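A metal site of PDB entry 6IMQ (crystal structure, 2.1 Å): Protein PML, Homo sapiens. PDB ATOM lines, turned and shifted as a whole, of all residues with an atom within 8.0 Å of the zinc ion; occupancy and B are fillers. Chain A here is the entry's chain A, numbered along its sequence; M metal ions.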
ATOM      1  N   TRP A  22     -19.621  22.353 -15.841  1.00  0.00           N
ATOM      2  CA  TRP A  22     -19.541  21.075 -15.152  1.00  0.00           C
ATOM      3  C   TRP A  22     -19.697  19.952 -16.162  1.00  0.00           C
ATOM      4  O   TRP A  22     -20.679  19.929 -16.910  1.00  0.00           O
ATOM      5  CB  TRP A  22     -20.648  20.943 -14.100  1.00  0.00           C
ATOM      6  CG  TRP A  22     -20.774  19.581 -13.493  1.00  0.00           C
ATOM      7  CD1 TRP A  22     -21.680  18.614 -13.836  1.00  0.00           C
ATOM      8  CD2 TRP A  22     -19.966  19.035 -12.440  1.00  0.00           C
ATOM      9  NE1 TRP A  22     -21.482  17.500 -13.040  1.00  0.00           N
ATOM     10  CE2 TRP A  22     -20.436  17.732 -12.192  1.00  0.00           C
ATOM     11  CE3 TRP A  22     -18.884  19.521 -11.696  1.00  0.00           C
ATOM     12  CZ2 TRP A  22     -19.869  16.910 -11.223  1.00  0.00           C
ATOM     13  CZ3 TRP A  22     -18.332  18.705 -10.734  1.00  0.00           C
ATOM     14  CH2 TRP A  22     -18.822  17.418 -10.501  1.00  0.00           C
ATOM     15  N   CYS A  23     -18.762  19.010 -16.173  1.00  0.00           N
ATOM     16  CA  CYS A  23     -18.866  17.857 -17.072  1.00  0.00           C
ATOM     17  C   CYS A  23     -19.354  16.639 -16.292  1.00  0.00           C
ATOM     18  O   CYS A  23     -18.685  16.196 -15.346  1.00  0.00           O
ATOM     19  CB  CYS A  23     -17.542  17.530 -17.751  1.00  0.00           C
ATOM     20  SG  CYS A  23     -17.674  15.964 -18.685  1.00  0.00           S
ATOM     21  N   PHE A  24     -20.473  16.062 -16.731  1.00  0.00           N
ATOM     22  CA  PHE A  24     -21.058  14.952 -15.983  1.00  0.00           C
ATOM     23  C   PHE A  24     -20.230  13.688 -16.056  1.00  0.00           C
ATOM     24  O   PHE A  24     -20.314  12.842 -15.151  1.00  0.00           O
ATOM     25  CB  PHE A  24     -22.463  14.663 -16.504  1.00  0.00           C
ATOM     26  CG  PHE A  24     -23.479  15.665 -16.094  1.00  0.00           C
ATOM     27  CD1 PHE A  24     -24.008  15.622 -14.824  1.00  0.00           C
ATOM     28  CD2 PHE A  24     -23.868  16.665 -16.957  1.00  0.00           C
ATOM     29  CE1 PHE A  24     -24.947  16.549 -14.426  1.00  0.00           C
ATOM     30  CE2 PHE A  24     -24.798  17.597 -16.560  1.00  0.00           C
ATOM     31  CZ  PHE A  24     -25.332  17.540 -15.290  1.00  0.00           C
ATOM     32  N   GLU A  25     -19.456  13.502 -17.118  1.00  0.00           N
ATOM     33  CA  GLU A  25     -18.653  12.287 -17.213  1.00  0.00           C
ATOM     34  C   GLU A  25     -17.270  12.461 -16.596  1.00  0.00           C
ATOM     35  O   GLU A  25     -16.770  11.536 -15.952  1.00  0.00           O
ATOM     36  CB  GLU A  25     -18.553  11.849 -18.674  1.00  0.00           C
ATOM     37  CG  GLU A  25     -19.809  11.145 -19.161  1.00  0.00           C
ATOM     38  CD  GLU A  25     -20.305  11.696 -20.486  1.00  0.00           C
ATOM     39  OE1 GLU A  25     -20.788  12.850 -20.519  1.00  0.00           O
ATOM     40  OE2 GLU A  25     -20.208  10.968 -21.495  1.00  0.00           O
ATOM     41  N   CYS A  26     -16.647  13.626 -16.753  1.00  0.00           N
ATOM     42  CA  CYS A  26     -15.428  13.906 -16.014  1.00  0.00           C
ATOM     43  C   CYS A  26     -15.722  14.145 -14.525  1.00  0.00           C
ATOM     44  O   CYS A  26     -14.870  13.875 -13.679  1.00  0.00           O
ATOM     45  CB  CYS A  26     -14.683  15.095 -16.631  1.00  0.00           C
ATOM     46  SG  CYS A  26     -14.092  14.905 -18.364  1.00  0.00           S
ATOM     47  N   GLU A  27     -16.941  14.591 -14.203  1.00  0.00           N
ATOM     48  CA  GLU A  27     -17.278  15.032 -12.840  1.00  0.00           C
ATOM     49  C   GLU A  27     -16.277  16.073 -12.375  1.00  0.00           C
ATOM     50  O   GLU A  27     -15.565  15.915 -11.379  1.00  0.00           O
ATOM     51  CB  GLU A  27     -17.331  13.845 -11.862  1.00  0.00           C
ATOM     52  CG  GLU A  27     -18.082  12.625 -12.391  1.00  0.00           C
ATOM     53  CD  GLU A  27     -19.358  12.315 -11.610  1.00  0.00           C
ATOM     54  OE1 GLU A  27     -19.296  11.599 -10.588  1.00  0.00           O
ATOM     55  OE2 GLU A  27     -20.436  12.800 -12.036  1.00  0.00           O
ATOM     56  N   GLN A  28     -16.215  17.160 -13.139  1.00  0.00           N
ATOM     57  CA  GLN A  28     -15.193  18.168 -12.937  1.00  0.00           C
ATOM     58  C   GLN A  28     -15.769  19.547 -13.216  1.00  0.00           C
ATOM     59  O   GLN A  28     -16.569  19.700 -14.145  1.00  0.00           O
ATOM     60  CB  GLN A  28     -14.003  18.007 -13.880  1.00  0.00           C
ATOM     61  CG  GLN A  28     -12.922  17.096 -13.466  1.00  0.00           C
ATOM     62  CD  GLN A  28     -11.834  16.969 -14.540  1.00  0.00           C
ATOM     63  OE1 GLN A  28     -11.366  17.998 -15.049  1.00  0.00           O
ATOM     64  NE2 GLN A  28     -11.613  15.763 -15.036  1.00  0.00           N
ATOM     65  N   LEU A  30     -14.745  23.162 -14.724  1.00  0.00           N
ATOM     66  CA  LEU A  30     -13.758  23.694 -15.654  1.00  0.00           C
ATOM     67  C   LEU A  30     -14.037  25.162 -15.971  1.00  0.00           C
ATOM     68  O   LEU A  30     -15.186  25.563 -16.156  1.00  0.00           O
ATOM     69  CB  LEU A  30     -13.764  22.861 -16.940  1.00  0.00           C
ATOM     70  CG  LEU A  30     -13.438  21.392 -16.693  1.00  0.00           C
ATOM     71  CD1 LEU A  30     -13.750  20.525 -17.904  1.00  0.00           C
ATOM     72  CD2 LEU A  30     -11.956  21.228 -16.292  1.00  0.00           C
ATOM     73  N   PHE A  35     -12.421  24.238 -20.604  1.00  0.00           N
ATOM     74  CA  PHE A  35     -13.516  23.504 -21.216  1.00  0.00           C
ATOM     75  C   PHE A  35     -13.375  23.469 -22.738  1.00  0.00           C
ATOM     76  O   PHE A  35     -13.718  22.464 -23.364  1.00  0.00           O
ATOM     77  CB  PHE A  35     -14.884  24.075 -20.843  1.00  0.00           C
ATOM     78  CG  PHE A  35     -16.027  23.227 -21.304  1.00  0.00           C
ATOM     79  CD1 PHE A  35     -16.243  21.969 -20.762  1.00  0.00           C
ATOM     80  CD2 PHE A  35     -16.891  23.671 -22.295  1.00  0.00           C
ATOM     81  CE1 PHE A  35     -17.283  21.171 -21.197  1.00  0.00           C
ATOM     82  CE2 PHE A  35     -17.944  22.878 -22.727  1.00  0.00           C
ATOM     83  CZ  PHE A  35     -18.127  21.623 -22.180  1.00  0.00           C
ATOM     84  N   HIS A  38     -11.199  20.727 -23.339  1.00  0.00           N
ATOM     85  CA  HIS A  38     -12.026  19.542 -23.125  1.00  0.00           C
ATOM     86  C   HIS A  38     -12.813  19.173 -24.373  1.00  0.00           C
ATOM     87  O   HIS A  38     -12.843  18.010 -24.787  1.00  0.00           O
ATOM     88  CB  HIS A  38     -12.955  19.793 -21.936  1.00  0.00           C
ATOM     89  CG  HIS A  38     -13.927  18.701 -21.666  1.00  0.00           C
ATOM     90  ND1 HIS A  38     -15.169  18.661 -22.265  1.00  0.00           N
ATOM     91  CD2 HIS A  38     -13.862  17.616 -20.853  1.00  0.00           C
ATOM     92  CE1 HIS A  38     -15.832  17.596 -21.835  1.00  0.00           C
ATOM     93  NE2 HIS A  38     -15.057  16.939 -20.981  1.00  0.00           N
ATOM     94  N   GLN A  39     -13.463  20.163 -25.004  1.00  0.00           N
ATOM     95  CA  GLN A  39     -14.297  19.879 -26.163  1.00  0.00           C
ATOM     96  C   GLN A  39     -13.470  19.455 -27.371  1.00  0.00           C
ATOM     97  O   GLN A  39     -13.965  18.735 -28.237  1.00  0.00           O
ATOM     98  CB  GLN A  39     -15.122  21.114 -26.543  1.00  0.00           C
ATOM     99  CG  GLN A  39     -16.105  21.541 -25.480  1.00  0.00           C
ATOM    100  CD  GLN A  39     -17.180  20.498 -25.236  1.00  0.00           C
ATOM    101  OE1 GLN A  39     -16.933  19.467 -24.606  1.00  0.00           O
ATOM    102  NE2 GLN A  39     -18.382  20.774 -25.720  1.00  0.00           N
ATOM    103  N   LEU A  42     -12.684  15.577 -26.350  1.00  0.00           N
ATOM    104  CA  LEU A  42     -13.728  14.697 -25.831  1.00  0.00           C
ATOM    105  C   LEU A  42     -15.096  15.182 -26.274  1.00  0.00           C
ATOM    106  O   LEU A  42     -15.289  16.344 -26.647  1.00  0.00           O
ATOM    107  CB  LEU A  42     -13.680  14.634 -24.303  1.00  0.00           C
ATOM    108  CG  LEU A  42     -12.363  14.143 -23.698  1.00  0.00           C
ATOM    109  CD1 LEU A  42     -12.239  14.661 -22.281  1.00  0.00           C
ATOM    110  CD2 LEU A  42     -12.335  12.630 -23.737  1.00  0.00           C
ATOM    111  N   LYS A  43     -16.079  14.273 -26.199  1.00  0.00           N
ATOM    112  CA  LYS A  43     -17.490  14.601 -26.353  1.00  0.00           C
ATOM    113  C   LYS A  43     -18.252  14.020 -25.163  1.00  0.00           C
ATOM    114  O   LYS A  43     -18.545  12.820 -25.132  1.00  0.00           O
ATOM    115  CB  LYS A  43     -18.033  14.062 -27.673  1.00  0.00           C
ATOM    116  CG  LYS A  43     -19.555  14.030 -27.810  1.00  0.00           C
ATOM    117  CD  LYS A  43     -19.961  13.423 -29.162  1.00  0.00           C
ATOM    118  CE  LYS A  43     -19.915  11.886 -29.146  1.00  0.00           C
ATOM    119  NZ  LYS A  43     -21.139  11.239 -29.695  1.00  0.00           N
ATOM    120  N   HIS A  44     -18.626  14.896 -24.231  1.00  0.00           N
ATOM    121  CA  HIS A  44     -19.251  14.495 -22.978  1.00  0.00           C
ATOM    122  C   HIS A  44     -20.473  15.369 -22.715  1.00  0.00           C
ATOM    123  O   HIS A  44     -20.588  16.489 -23.219  1.00  0.00           O
ATOM    124  CB  HIS A  44     -18.294  14.647 -21.773  1.00  0.00           C
ATOM    125  CG  HIS A  44     -17.172  13.645 -21.742  1.00  0.00           C
ATOM    126  ND1 HIS A  44     -16.133  13.742 -20.834  1.00  0.00           N
ATOM    127  CD2 HIS A  44     -16.934  12.545 -22.486  1.00  0.00           C
ATOM    128  CE1 HIS A  44     -15.302  12.730 -21.016  1.00  0.00           C
ATOM    129  NE2 HIS A  44     -15.754  11.997 -22.014  1.00  0.00           N
ATOM    130  N   GLU A  45     -21.375  14.866 -21.870  1.00  0.00           N
ATOM    131  CA  GLU A  45     -22.505  15.676 -21.396  1.00  0.00           C
ATOM    132  C   GLU A  45     -21.998  16.707 -20.389  1.00  0.00           C
ATOM    133  O   GLU A  45     -21.379  16.342 -19.386  1.00  0.00           O
ATOM    134  CB  GLU A  45     -23.578  14.797 -20.769  1.00  0.00           C
ATOM    135  CG  GLU A  45     -24.593  14.253 -21.766  1.00  0.00           C
ATOM    136  CD  GLU A  45     -25.137  15.331 -22.694  1.00  0.00           C
ATOM    137  OE1 GLU A  45     -25.338  16.484 -22.228  1.00  0.00           O
ATOM    138  OE2 GLU A  45     -25.330  15.040 -23.882  1.00  0.00           O
ATOM    139  N   ALA A  46     -22.259  17.978 -20.667  1.00  0.00           N
ATOM    140  CA  ALA A  46     -21.794  19.074 -19.820  1.00  0.00           C
ATOM    141  C   ALA A  46     -22.772  20.233 -19.892  1.00  0.00           C
ATOM    142  O   ALA A  46     -23.566  20.345 -20.826  1.00  0.00           O
ATOM    143  CB  ALA A  46     -20.393  19.539 -20.241  1.00  0.00           C
HETATM  144 ZN    ZN M   1     -15.755  15.559 -19.788  1.00  0.00          ZN
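The side-chain sulfur (SG) of Cys 23 sits close to the backbone NH (N) of Glu 25, at 3.4 Å. A ring nitrogen (ND1) of His 38 is in hydrogen-bond range of the side-chain amide oxygen (OE1) of Gln 39 (3.0 Å). The backbone NH (N) of Cys 23 lies within hydrogen-bond range of the backbone carbonyl oxygen (O) of Gln 28. The side-chain sulfur (SG) of Cys 23 sits close to the backbone carbonyl oxygen (O) of Glu 45 (3.8 Å).
Within 4 Å of the zinc ion: Cys 23, Cys 26, His 38 and His 44.
The zinc ion is bound by a ring nitrogen (NE2) of His 38 (2.0 Å), a ring nitrogen (ND1) of His 44 (2.1 Å), the side-chain sulfur (SG) of Cys 23 (2.3 Å) and the side-chain sulfur (SG) of Cys 26 (2.3 Å).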
